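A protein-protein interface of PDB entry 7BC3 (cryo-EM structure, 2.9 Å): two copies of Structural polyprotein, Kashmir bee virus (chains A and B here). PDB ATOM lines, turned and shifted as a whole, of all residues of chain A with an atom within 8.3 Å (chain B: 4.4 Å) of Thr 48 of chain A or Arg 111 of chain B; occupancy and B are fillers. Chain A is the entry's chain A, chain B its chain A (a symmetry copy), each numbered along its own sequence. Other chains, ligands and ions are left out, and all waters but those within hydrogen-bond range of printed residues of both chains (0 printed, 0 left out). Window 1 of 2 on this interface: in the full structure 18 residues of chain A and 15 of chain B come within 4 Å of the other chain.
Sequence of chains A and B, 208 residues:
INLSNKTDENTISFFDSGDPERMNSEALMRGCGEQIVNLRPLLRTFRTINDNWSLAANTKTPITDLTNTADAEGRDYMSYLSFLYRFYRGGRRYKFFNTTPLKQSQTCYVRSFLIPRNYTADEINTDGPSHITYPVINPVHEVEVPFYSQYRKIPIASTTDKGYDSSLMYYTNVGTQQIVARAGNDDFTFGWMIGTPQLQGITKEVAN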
ATOM      1  N   THR A  45      -1.907  13.993 -24.693  1.00  0.00           N
ATOM      2  CA  THR A  45      -2.403  12.910 -23.865  1.00  0.00           C
ATOM      3  C   THR A  45      -1.606  12.824 -22.572  1.00  0.00           C
ATOM      4  O   THR A  45      -0.457  13.269 -22.495  1.00  0.00           O
ATOM      5  CB  THR A  45      -2.309  11.572 -24.598  1.00  0.00           C
ATOM      6  OG1 THR A  45      -0.932  11.250 -24.826  1.00  0.00           O
ATOM      7  CG2 THR A  45      -3.031  11.630 -25.922  1.00  0.00           C
ATOM      8  N   PHE A  46      -2.224  12.237 -21.556  1.00  0.00           N
ATOM      9  CA  PHE A  46      -1.571  12.000 -20.279  1.00  0.00           C
ATOM     10  C   PHE A  46      -1.150  10.544 -20.194  1.00  0.00           C
ATOM     11  O   PHE A  46      -1.947   9.642 -20.472  1.00  0.00           O
ATOM     12  CB  PHE A  46      -2.496  12.352 -19.116  1.00  0.00           C
ATOM     13  CG  PHE A  46      -2.557  13.814 -18.822  1.00  0.00           C
ATOM     14  CD1 PHE A  46      -1.769  14.367 -17.832  1.00  0.00           C
ATOM     15  CD2 PHE A  46      -3.396  14.640 -19.541  1.00  0.00           C
ATOM     16  CE1 PHE A  46      -1.821  15.712 -17.565  1.00  0.00           C
ATOM     17  CE2 PHE A  46      -3.452  15.986 -19.276  1.00  0.00           C
ATOM     18  CZ  PHE A  46      -2.663  16.523 -18.286  1.00  0.00           C
ATOM     19  N   ARG A  47       0.102  10.322 -19.812  1.00  0.00           N
ATOM     20  CA  ARG A  47       0.640   8.983 -19.655  1.00  0.00           C
ATOM     21  C   ARG A  47       1.414   8.925 -18.351  1.00  0.00           C
ATOM     22  O   ARG A  47       1.953   9.929 -17.882  1.00  0.00           O
ATOM     23  CB  ARG A  47       1.540   8.585 -20.827  1.00  0.00           C
ATOM     24  CG  ARG A  47       0.786   8.371 -22.120  1.00  0.00           C
ATOM     25  CD  ARG A  47       0.240   6.961 -22.216  1.00  0.00           C
ATOM     26  NE  ARG A  47      -0.453   6.729 -23.478  1.00  0.00           N
ATOM     27  CZ  ARG A  47      -1.662   7.202 -23.762  1.00  0.00           C
ATOM     28  NH1 ARG A  47      -2.320   7.935 -22.878  1.00  0.00           N
ATOM     29  NH2 ARG A  47      -2.216   6.944 -24.937  1.00  0.00           N
ATOM     30  N   THR A  48       1.456   7.735 -17.772  1.00  0.00           N
ATOM     31  CA  THR A  48       2.016   7.556 -16.445  1.00  0.00           C
ATOM     32  C   THR A  48       3.536   7.513 -16.499  1.00  0.00           C
ATOM     33  O   THR A  48       4.123   6.886 -17.387  1.00  0.00           O
ATOM     34  CB  THR A  48       1.470   6.277 -15.825  1.00  0.00           C
ATOM     35  OG1 THR A  48       0.043   6.349 -15.797  1.00  0.00           O
ATOM     36  CG2 THR A  48       1.990   6.092 -14.420  1.00  0.00           C
ATOM     37  N   ILE A  49       4.165   8.190 -15.544  1.00  0.00           N
ATOM     38  CA  ILE A  49       5.607   8.125 -15.367  1.00  0.00           C
ATOM     39  C   ILE A  49       5.992   7.469 -14.049  1.00  0.00           C
ATOM     40  O   ILE A  49       7.170   7.118 -13.874  1.00  0.00           O
ATOM     41  CB  ILE A  49       6.242   9.526 -15.472  1.00  0.00           C
ATOM     42  CG1 ILE A  49       5.802  10.401 -14.301  1.00  0.00           C
ATOM     43  CG2 ILE A  49       5.843  10.180 -16.775  1.00  0.00           C
ATOM     44  CD1 ILE A  49       6.174  11.849 -14.454  1.00  0.00           C
ATOM     45  N   ASN A  50       5.050   7.295 -13.124  1.00  0.00           N
ATOM     46  CA  ASN A  50       5.313   6.599 -11.873  1.00  0.00           C
ATOM     47  C   ASN A  50       3.982   6.237 -11.235  1.00  0.00           C
ATOM     48  O   ASN A  50       3.118   7.102 -11.077  1.00  0.00           O
ATOM     49  CB  ASN A  50       6.151   7.461 -10.924  1.00  0.00           C
ATOM     50  CG  ASN A  50       6.640   6.692  -9.715  1.00  0.00           C
ATOM     51  OD1 ASN A  50       5.984   5.765  -9.245  1.00  0.00           O
ATOM     52  ND2 ASN A  50       7.806   7.072  -9.207  1.00  0.00           N
ATOM     53  N   ASP A  51       3.820   4.965 -10.880  1.00  0.00           N
ATOM     54  CA  ASP A  51       2.614   4.497 -10.210  1.00  0.00           C
ATOM     55  C   ASP A  51       2.670   4.668  -8.701  1.00  0.00           C
ATOM     56  O   ASP A  51       1.629   4.569  -8.043  1.00  0.00           O
ATOM     57  CB  ASP A  51       2.363   3.018 -10.530  1.00  0.00           C
ATOM     58  CG  ASP A  51       1.948   2.782 -11.967  1.00  0.00           C
ATOM     59  OD1 ASP A  51       1.147   3.580 -12.498  1.00  0.00           O
ATOM     60  OD2 ASP A  51       2.426   1.796 -12.568  1.00  0.00           O
ATOM     61  N   ASN A  52       3.852   4.912  -8.138  1.00  0.00           N
ATOM     62  CA  ASN A  52       3.996   5.054  -6.692  1.00  0.00           C
ATOM     63  C   ASN A  52       5.141   6.027  -6.435  1.00  0.00           C
ATOM     64  O   ASN A  52       6.312   5.635  -6.470  1.00  0.00           O
ATOM     65  CB  ASN A  52       4.252   3.708  -6.030  1.00  0.00           C
ATOM     66  CG  ASN A  52       4.072   3.757  -4.529  1.00  0.00           C
ATOM     67  OD1 ASN A  52       5.023   3.565  -3.770  1.00  0.00           O
ATOM     68  ND2 ASN A  52       2.849   4.023  -4.090  1.00  0.00           N
ATOM     69  N   LEU A  66      11.945  13.627  -9.784  1.00  0.00           N
ATOM     70  CA  LEU A  66      11.313  12.513 -10.478  1.00  0.00           C
ATOM     71  C   LEU A  66      11.512  12.579 -11.986  1.00  0.00           C
ATOM     72  O   LEU A  66      11.872  11.576 -12.619  1.00  0.00           O
ATOM     73  CB  LEU A  66       9.817  12.501 -10.157  1.00  0.00           C
ATOM     74  CG  LEU A  66       8.965  11.424 -10.825  1.00  0.00           C
ATOM     75  CD1 LEU A  66       9.284  10.059 -10.249  1.00  0.00           C
ATOM     76  CD2 LEU A  66       7.498  11.757 -10.654  1.00  0.00           C
ATOM     77  N   ALA A  70      12.502  10.024 -15.078  1.00  0.00           N
ATOM     78  CA  ALA A  70      11.404   9.663 -15.965  1.00  0.00           C
ATOM     79  C   ALA A  70      11.642  10.104 -17.407  1.00  0.00           C
ATOM     80  O   ALA A  70      11.009   9.565 -18.319  1.00  0.00           O
ATOM     81  CB  ALA A  70      10.100  10.260 -15.431  1.00  0.00           C
ATOM     82  N   GLU A  73      14.300   7.375 -18.801  1.00  0.00           N
ATOM     83  CA  GLU A  73      13.741   6.034 -18.940  1.00  0.00           C
ATOM     84  C   GLU A  73      13.193   5.803 -20.344  1.00  0.00           C
ATOM     85  O   GLU A  73      13.592   4.856 -21.030  1.00  0.00           O
ATOM     86  CB  GLU A  73      12.653   5.811 -17.891  1.00  0.00           C
ATOM     87  CG  GLU A  73      13.189   5.293 -16.570  1.00  0.00           C
ATOM     88  CD  GLU A  73      12.146   5.291 -15.473  1.00  0.00           C
ATOM     89  OE1 GLU A  73      11.012   5.747 -15.727  1.00  0.00           O
ATOM     90  OE2 GLU A  73      12.461   4.832 -14.356  1.00  0.00           O
ATOM     91  N   GLY A  74      12.279   6.662 -20.790  1.00  0.00           N
ATOM     92  CA  GLY A  74      11.640   6.490 -22.080  1.00  0.00           C
ATOM     93  C   GLY A  74      10.296   5.807 -22.038  1.00  0.00           C
ATOM     94  O   GLY A  74       9.859   5.268 -23.061  1.00  0.00           O
ATOM     95  N   ARG A  75       9.620   5.814 -20.889  1.00  0.00           N
ATOM     96  CA  ARG A  75       8.349   5.112 -20.761  1.00  0.00           C
ATOM     97  C   ARG A  75       7.192   5.952 -21.280  1.00  0.00           C
ATOM     98  O   ARG A  75       6.291   5.427 -21.944  1.00  0.00           O
ATOM     99  CB  ARG A  75       8.124   4.730 -19.299  1.00  0.00           C
ATOM    100  CG  ARG A  75       6.874   3.909 -19.041  1.00  0.00           C
ATOM    101  CD  ARG A  75       6.424   4.034 -17.598  1.00  0.00           C
ATOM    102  NE  ARG A  75       5.047   3.590 -17.413  1.00  0.00           N
ATOM    103  CZ  ARG A  75       4.473   3.417 -16.227  1.00  0.00           C
ATOM    104  NH1 ARG A  75       5.156   3.651 -15.114  1.00  0.00           N
ATOM    105  NH2 ARG A  75       3.214   3.009 -16.153  1.00  0.00           N
ATOM    106  N   ASP A  76       7.195   7.247 -20.990  1.00  0.00           N
ATOM    107  CA  ASP A  76       6.147   8.140 -21.453  1.00  0.00           C
ATOM    108  C   ASP A  76       6.490   8.693 -22.833  1.00  0.00           C
ATOM    109  O   ASP A  76       7.596   8.520 -23.349  1.00  0.00           O
ATOM    110  CB  ASP A  76       5.935   9.279 -20.458  1.00  0.00           C
ATOM    111  CG  ASP A  76       7.202  10.059 -20.186  1.00  0.00           C
ATOM    112  OD1 ASP A  76       8.276   9.430 -20.086  1.00  0.00           O
ATOM    113  OD2 ASP A  76       7.125  11.300 -20.072  1.00  0.00           O
ATOM    114  N   TYR A  77       5.513   9.374 -23.433  1.00  0.00           N
ATOM    115  CA  TYR A  77       5.704   9.917 -24.771  1.00  0.00           C
ATOM    116  C   TYR A  77       6.545  11.185 -24.751  1.00  0.00           C
ATOM    117  O   TYR A  77       7.269  11.462 -25.713  1.00  0.00           O
ATOM    118  CB  TYR A  77       4.349  10.189 -25.420  1.00  0.00           C
ATOM    119  CG  TYR A  77       3.507   8.948 -25.632  1.00  0.00           C
ATOM    120  CD1 TYR A  77       4.090   7.692 -25.715  1.00  0.00           C
ATOM    121  CD2 TYR A  77       2.128   9.035 -25.749  1.00  0.00           C
ATOM    122  CE1 TYR A  77       3.327   6.564 -25.907  1.00  0.00           C
ATOM    123  CE2 TYR A  77       1.357   7.910 -25.945  1.00  0.00           C
ATOM    124  CZ  TYR A  77       1.962   6.676 -26.023  1.00  0.00           C
ATOM    125  OH  TYR A  77       1.205   5.546 -26.216  1.00  0.00           O
ATOM    126  N   LYS A  95      -0.664  15.462 -13.416  1.00  0.00           N
ATOM    127  CA  LYS A  95      -1.777  14.985 -12.613  1.00  0.00           C
ATOM    128  C   LYS A  95      -1.244  14.046 -11.547  1.00  0.00           C
ATOM    129  O   LYS A  95      -0.372  13.214 -11.819  1.00  0.00           O
ATOM    130  CB  LYS A  95      -2.819  14.260 -13.462  1.00  0.00           C
ATOM    131  CG  LYS A  95      -3.585  15.145 -14.412  1.00  0.00           C
ATOM    132  CD  LYS A  95      -4.854  14.461 -14.862  1.00  0.00           C
ATOM    133  CE  LYS A  95      -5.434  15.084 -16.115  1.00  0.00           C
ATOM    134  NZ  LYS A  95      -5.541  16.561 -16.034  1.00  0.00           N
ATOM    135  N   PHE A  97      -2.662  11.372  -8.887  1.00  0.00           N
ATOM    136  CA  PHE A  97      -3.752  10.555  -8.377  1.00  0.00           C
ATOM    137  C   PHE A  97      -3.335   9.970  -7.035  1.00  0.00           C
ATOM    138  O   PHE A  97      -2.297   9.307  -6.936  1.00  0.00           O
ATOM    139  CB  PHE A  97      -4.110   9.446  -9.363  1.00  0.00           C
ATOM    140  CG  PHE A  97      -4.410   9.936 -10.746  1.00  0.00           C
ATOM    141  CD1 PHE A  97      -5.715  10.138 -11.152  1.00  0.00           C
ATOM    142  CD2 PHE A  97      -3.390  10.189 -11.644  1.00  0.00           C
ATOM    143  CE1 PHE A  97      -5.995  10.586 -12.423  1.00  0.00           C
ATOM    144  CE2 PHE A  97      -3.668  10.638 -12.914  1.00  0.00           C
ATOM    145  CZ  PHE A  97      -4.970  10.837 -13.303  1.00  0.00           C
ATOM    146  N   THR A  99      -2.850   7.705  -3.893  1.00  0.00           N
ATOM    147  CA  THR A  99      -2.762   6.275  -3.627  1.00  0.00           C
ATOM    148  C   THR A  99      -2.288   6.042  -2.200  1.00  0.00           C
ATOM    149  O   THR A  99      -1.551   5.096  -1.910  1.00  0.00           O
ATOM    150  CB  THR A  99      -1.833   5.595  -4.630  1.00  0.00           C
ATOM    151  OG1 THR A  99      -2.228   5.944  -5.962  1.00  0.00           O
ATOM    152  CG2 THR A  99      -1.876   4.086  -4.478  1.00  0.00           C
ATOM    153  N   GLN A 178       1.398   8.639  -4.718  1.00  0.00           N
ATOM    154  CA  GLN A 178       0.632   9.162  -5.836  1.00  0.00           C
ATOM    155  C   GLN A 178       1.049   8.499  -7.138  1.00  0.00           C
ATOM    156  O   GLN A 178       2.206   8.104  -7.304  1.00  0.00           O
ATOM    157  CB  GLN A 178       0.816  10.679  -5.965  1.00  0.00           C
ATOM    158  CG  GLN A 178       0.359  11.470  -4.753  1.00  0.00           C
ATOM    159  CD  GLN A 178       0.939  12.863  -4.722  1.00  0.00           C
ATOM    160  OE1 GLN A 178       0.210  13.852  -4.668  1.00  0.00           O
ATOM    161  NE2 GLN A 178       2.262  12.949  -4.753  1.00  0.00           N
ATOM    162  N   ILE A 179       0.092   8.382  -8.051  1.00  0.00           N
ATOM    163  CA  ILE A 179       0.371   8.061  -9.445  1.00  0.00           C
ATOM    164  C   ILE A 179       0.556   9.379 -10.180  1.00  0.00           C
ATOM    165  O   ILE A 179      -0.320  10.250 -10.137  1.00  0.00           O
ATOM    166  CB  ILE A 179      -0.764   7.240 -10.074  1.00  0.00           C
ATOM    167  CG1 ILE A 179      -0.931   5.898  -9.365  1.00  0.00           C
ATOM    168  CG2 ILE A 179      -0.500   7.021 -11.548  1.00  0.00           C
ATOM    169  CD1 ILE A 179      -2.303   5.307  -9.541  1.00  0.00           C
ATOM    170  N   VAL A 180       1.690   9.535 -10.851  1.00  0.00           N
ATOM    171  CA  VAL A 180       2.031  10.774 -11.535  1.00  0.00           C
ATOM    172  C   VAL A 180       1.887  10.554 -13.032  1.00  0.00           C
ATOM    173  O   VAL A 180       2.524   9.660 -13.603  1.00  0.00           O
ATOM    174  CB  VAL A 180       3.447  11.249 -11.184  1.00  0.00           C
ATOM    175  CG1 VAL A 180       3.654  12.666 -11.679  1.00  0.00           C
ATOM    176  CG2 VAL A 180       3.678  11.166  -9.689  1.00  0.00           C
ATOM    177  N   ALA A 181       1.048  11.369 -13.658  1.00  0.00           N
ATOM    178  CA  ALA A 181       0.916  11.427 -15.104  1.00  0.00           C
ATOM    179  C   ALA A 181       1.192  12.850 -15.553  1.00  0.00           C
ATOM    180  O   ALA A 181       0.738  13.807 -14.920  1.00  0.00           O
ATOM    181  CB  ALA A 181      -0.477  11.000 -15.560  1.00  0.00           C
ATOM    182  N   ARG A 182       1.937  12.991 -16.643  1.00  0.00           N
ATOM    183  CA  ARG A 182       2.289  14.297 -17.166  1.00  0.00           C
ATOM    184  C   ARG A 182       1.890  14.389 -18.629  1.00  0.00           C
ATOM    185  O   ARG A 182       1.475  13.410 -19.254  1.00  0.00           O
ATOM    186  CB  ARG A 182       3.787  14.586 -17.006  1.00  0.00           C
ATOM    187  CG  ARG A 182       4.684  13.726 -17.861  1.00  0.00           C
ATOM    188  CD  ARG A 182       6.111  14.210 -17.785  1.00  0.00           C
ATOM    189  NE  ARG A 182       7.028  13.330 -18.497  1.00  0.00           N
ATOM    190  CZ  ARG A 182       8.334  13.541 -18.596  1.00  0.00           C
ATOM    191  NH1 ARG A 182       8.880  14.607 -18.030  1.00  0.00           N
ATOM    192  NH2 ARG A 182       9.095  12.688 -19.262  1.00  0.00           N
ATOM    193  N   ALA A 183       2.023  15.595 -19.166  1.00  0.00           N
ATOM    194  CA  ALA A 183       1.705  15.878 -20.556  1.00  0.00           C
ATOM    195  C   ALA A 183       2.110  17.316 -20.834  1.00  0.00           C
ATOM    196  O   ALA A 183       2.577  18.033 -19.946  1.00  0.00           O
ATOM    197  CB  ALA A 183       0.225  15.658 -20.854  1.00  0.00           C
ATOM    198  N   TYR B 109      -8.659   2.362  -5.007  1.00  0.00           N
ATOM    199  CA  TYR B 109      -8.759   2.876  -6.362  1.00  0.00           C
ATOM    200  C   TYR B 109      -8.790   1.716  -7.343  1.00  0.00           C
ATOM    201  O   TYR B 109      -8.191   0.663  -7.111  1.00  0.00           O
ATOM    202  CB  TYR B 109      -7.605   3.834  -6.699  1.00  0.00           C
ATOM    203  CG  TYR B 109      -6.275   3.174  -6.984  1.00  0.00           C
ATOM    204  CD1 TYR B 109      -5.332   3.016  -5.983  1.00  0.00           C
ATOM    205  CD2 TYR B 109      -5.953   2.738  -8.259  1.00  0.00           C
ATOM    206  CE1 TYR B 109      -4.116   2.424  -6.238  1.00  0.00           C
ATOM    207  CE2 TYR B 109      -4.740   2.145  -8.523  1.00  0.00           C
ATOM    208  CZ  TYR B 109      -3.823   1.990  -7.510  1.00  0.00           C
ATOM    209  OH  TYR B 109      -2.607   1.402  -7.768  1.00  0.00           O
ATOM    210  N   VAL B 110      -9.503   1.928  -8.443  1.00  0.00           N
ATOM    211  CA  VAL B 110      -9.677   0.935  -9.493  1.00  0.00           C
ATOM    212  C   VAL B 110      -9.087   1.490 -10.776  1.00  0.00           C
ATOM    213  O   VAL B 110      -9.191   2.690 -11.048  1.00  0.00           O
ATOM    214  CB  VAL B 110     -11.160   0.572  -9.693  1.00  0.00           C
ATOM    215  CG1 VAL B 110     -11.329  -0.276 -10.930  1.00  0.00           C
ATOM    216  CG2 VAL B 110     -11.694  -0.143  -8.474  1.00  0.00           C
ATOM    217  N   ARG B 111      -8.480   0.613 -11.568  1.00  0.00           N
ATOM    218  CA  ARG B 111      -7.778   1.025 -12.770  1.00  0.00           C
ATOM    219  C   ARG B 111      -7.997  -0.001 -13.868  1.00  0.00           C
ATOM    220  O   ARG B 111      -7.982  -1.208 -13.615  1.00  0.00           O
ATOM    221  CB  ARG B 111      -6.287   1.190 -12.493  1.00  0.00           C
ATOM    222  CG  ARG B 111      -5.620   2.211 -13.360  1.00  0.00           C
ATOM    223  CD  ARG B 111      -4.285   2.598 -12.789  1.00  0.00           C
ATOM    224  NE  ARG B 111      -3.499   3.345 -13.756  1.00  0.00           N
ATOM    225  CZ  ARG B 111      -2.176   3.425 -13.744  1.00  0.00           C
ATOM    226  NH1 ARG B 111      -1.470   2.807 -12.807  1.00  0.00           N
ATOM    227  NH2 ARG B 111      -1.558   4.126 -14.674  1.00  0.00           N
ATOM    228  N   SER B 112      -8.198   0.491 -15.088  1.00  0.00           N
ATOM    229  CA  SER B 112      -8.438  -0.353 -16.248  1.00  0.00           C
ATOM    230  C   SER B 112      -7.454   0.003 -17.349  1.00  0.00           C
ATOM    231  O   SER B 112      -7.202   1.182 -17.616  1.00  0.00           O
ATOM    232  CB  SER B 112      -9.868  -0.197 -16.763  1.00  0.00           C
ATOM    233  OG  SER B 112     -10.052   1.060 -17.385  1.00  0.00           O
ATOM    234  N   PHE B 113      -6.905  -1.025 -17.988  1.00  0.00           N
ATOM    235  CA  PHE B 113      -5.948  -0.867 -19.068  1.00  0.00           C
ATOM    236  C   PHE B 113      -6.444  -1.624 -20.291  1.00  0.00           C
ATOM    237  O   PHE B 113      -7.412  -2.387 -20.232  1.00  0.00           O
ATOM    238  CB  PHE B 113      -4.562  -1.382 -18.663  1.00  0.00           C
ATOM    239  CG  PHE B 113      -4.065  -0.827 -17.366  1.00  0.00           C
ATOM    240  CD1 PHE B 113      -3.349   0.354 -17.335  1.00  0.00           C
ATOM    241  CD2 PHE B 113      -4.315  -1.486 -16.176  1.00  0.00           C
ATOM    242  CE1 PHE B 113      -2.889   0.865 -16.144  1.00  0.00           C
ATOM    243  CE2 PHE B 113      -3.859  -0.977 -14.983  1.00  0.00           C
ATOM    244  CZ  PHE B 113      -3.145   0.202 -14.967  1.00  0.00           C
ATOM    245  N   SER B 130      -5.707   4.631 -20.125  1.00  0.00           N
ATOM    246  CA  SER B 130      -6.196   4.015 -18.904  1.00  0.00           C
ATOM    247  C   SER B 130      -7.327   4.854 -18.339  1.00  0.00           C
ATOM    248  O   SER B 130      -7.516   6.015 -18.707  1.00  0.00           O
ATOM    249  CB  SER B 130      -5.079   3.866 -17.865  1.00  0.00           C
ATOM    250  OG  SER B 130      -5.549   3.200 -16.707  1.00  0.00           O
ATOM    251  N   HIS B 131      -8.082   4.243 -17.431  1.00  0.00           N
ATOM    252  CA  HIS B 131      -9.137   4.913 -16.691  1.00  0.00           C
ATOM    253  C   HIS B 131      -9.045   4.497 -15.234  1.00  0.00           C
ATOM    254  O   HIS B 131      -8.878   3.314 -14.927  1.00  0.00           O
ATOM    255  CB  HIS B 131     -10.521   4.576 -17.242  1.00  0.00           C
ATOM    256  CG  HIS B 131     -11.634   5.298 -16.551  1.00  0.00           C
ATOM    257  ND1 HIS B 131     -12.821   4.686 -16.211  1.00  0.00           N
ATOM    258  CD2 HIS B 131     -11.739   6.580 -16.130  1.00  0.00           C
ATOM    259  CE1 HIS B 131     -13.609   5.561 -15.613  1.00  0.00           C
ATOM    260  NE2 HIS B 131     -12.975   6.718 -15.551  1.00  0.00           N
ATOM    261  N   ILE B 132      -9.148   5.474 -14.340  1.00  0.00           N
ATOM    262  CA  ILE B 132      -9.012   5.249 -12.909  1.00  0.00           C
ATOM    263  C   ILE B 132     -10.218   5.845 -12.204  1.00  0.00           C
ATOM    264  O   ILE B 132     -10.663   6.949 -12.539  1.00  0.00           O
ATOM    265  CB  ILE B 132      -7.700   5.850 -12.361  1.00  0.00           C
ATOM    266  CG1 ILE B 132      -7.455   5.380 -10.931  1.00  0.00           C
ATOM    267  CG2 ILE B 132      -7.738   7.362 -12.418  1.00  0.00           C
ATOM    268  CD1 ILE B 132      -6.061   5.637 -10.444  1.00  0.00           C
ATOM    269  N   MET B 169      -7.968  -4.958 -19.420  1.00  0.00           N
ATOM    270  CA  MET B 169      -7.238  -5.432 -18.255  1.00  0.00           C
ATOM    271  C   MET B 169      -7.664  -4.598 -17.057  1.00  0.00           C
ATOM    272  O   MET B 169      -7.799  -3.375 -17.162  1.00  0.00           O
ATOM    273  CB  MET B 169      -5.728  -5.336 -18.465  1.00  0.00           C
ATOM    274  CG  MET B 169      -4.926  -6.274 -17.589  1.00  0.00           C
ATOM    275  SD  MET B 169      -3.222  -6.458 -18.135  1.00  0.00           S
ATOM    276  CE  MET B 169      -2.825  -4.763 -18.542  1.00  0.00           C
ATOM    277  N   TYR B 170      -7.874  -5.261 -15.927  1.00  0.00           N
ATOM    278  CA  TYR B 170      -8.458  -4.653 -14.741  1.00  0.00           C
ATOM    279  C   TYR B 170      -7.477  -4.787 -13.587  1.00  0.00           C
ATOM    280  O   TYR B 170      -6.902  -5.860 -13.378  1.00  0.00           O
ATOM    281  CB  TYR B 170      -9.786  -5.330 -14.413  1.00  0.00           C
ATOM    282  CG  TYR B 170     -10.813  -4.462 -13.729  1.00  0.00           C
ATOM    283  CD1 TYR B 170     -11.427  -3.413 -14.395  1.00  0.00           C
ATOM    284  CD2 TYR B 170     -11.196  -4.719 -12.426  1.00  0.00           C
ATOM    285  CE1 TYR B 170     -12.376  -2.632 -13.772  1.00  0.00           C
ATOM    286  CE2 TYR B 170     -12.143  -3.951 -11.794  1.00  0.00           C
ATOM    287  CZ  TYR B 170     -12.733  -2.910 -12.470  1.00  0.00           C
ATOM    288  OH  TYR B 170     -13.681  -2.139 -11.842  1.00  0.00           O
ATOM    289  N   TYR B 171      -7.285  -3.701 -12.843  1.00  0.00           N
ATOM    290  CA  TYR B 171      -6.327  -3.671 -11.752  1.00  0.00           C
ATOM    291  C   TYR B 171      -6.952  -2.987 -10.549  1.00  0.00           C
ATOM    292  O   TYR B 171      -7.781  -2.084 -10.688  1.00  0.00           O
ATOM    293  CB  TYR B 171      -5.037  -2.943 -12.150  1.00  0.00           C
ATOM    294  CG  TYR B 171      -4.039  -2.814 -11.025  1.00  0.00           C
ATOM    295  CD1 TYR B 171      -3.084  -3.794 -10.805  1.00  0.00           C
ATOM    296  CD2 TYR B 171      -4.051  -1.712 -10.183  1.00  0.00           C
ATOM    297  CE1 TYR B 171      -2.173  -3.680  -9.779  1.00  0.00           C
ATOM    298  CE2 TYR B 171      -3.146  -1.593  -9.154  1.00  0.00           C
ATOM    299  CZ  TYR B 171      -2.207  -2.579  -8.955  1.00  0.00           C
ATOM    300  OH  TYR B 171      -1.299  -2.462  -7.930  1.00  0.00           O
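Of the 11 printed residues of chain B, 3 touch a printed residue of chain A.
Hydrophobic or aromatic side chains of chain B within 4 Å of the printed part of chain A: Tyr 109 and Ile 132.
Among the printed residues, 5 pairs touch across the chains.
O of Arg 111 of chain B lies within hydrogen-bond range of N of Tyr 171 of chain B, 2.7 Å away.
The backbone carbonyl oxygen (O) of Phe 97 of chain A sits at hydrogen-bond distance from the backbone NH (N) of Ile 179 of chain A.
NE of Arg 75 of chain A is in hydrogen-bond range of O of Thr 48 of chain A (3.4 Å).
The side-chain carboxylate (OD2) of Asp 51 of chain A is in salt-bridge range of the guanidinium group (NH2) of Arg 75 of chain A.
No position is printed for both chains.
Of the 5 pairs that touch across the chains among the printed residues, none has its exchanged pair printed and touching as well.
Among the printed residues, pairs that only touch across the chains: Thr 99 of chain A with Tyr 109 of chain B (3.3 Å), Phe 97 of chain A with Ile 132 of chain B (3.7 Å) and Ile 179 of chain A with Ile 132 of chain B (3.9 Å).
The side-chain carboxylate of Asp 51 of chain A lies within salt-bridge range of the guanidinium group of Arg 111 of chain B, 2.7 Å away.
The side-chain hydroxyl of Thr 48 of chain A sits at hydrogen-bond distance from the guanidinium group of Arg 111 of chain B (3.0 Å).
Of chain B, only Arg 111 comes within 4 Å of Thr 48 of chain A.
No residue of chain A comes within 4 Å of Ser 112 of chain B.
Printed residues of chain B within 4 Å of Thr 99 of chain A: Tyr 109.
Printed residues of chain B within 4 Å of Asp 51 of chain A: Arg 111 (2.7 Å).
Of the printed residues of chain A, Tyr 109 of chain B touches Thr 99 (3.3 Å).
Of the printed residues of chain B, Phe 97 of chain A touches Ile 132 (3.7 Å).
The nearest printed residue of chain B that does not touch Thr 48 of chain A is Ser 130 of chain B (6.1 Å).
The nearest residue of chain A that does not touch Arg 111 of chain B is Ile 179 of chain A (4.2 Å).
The nearest printed residue of chain B that does not touch Ile 179 of chain A is Tyr 109 of chain B (4.1 Å).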
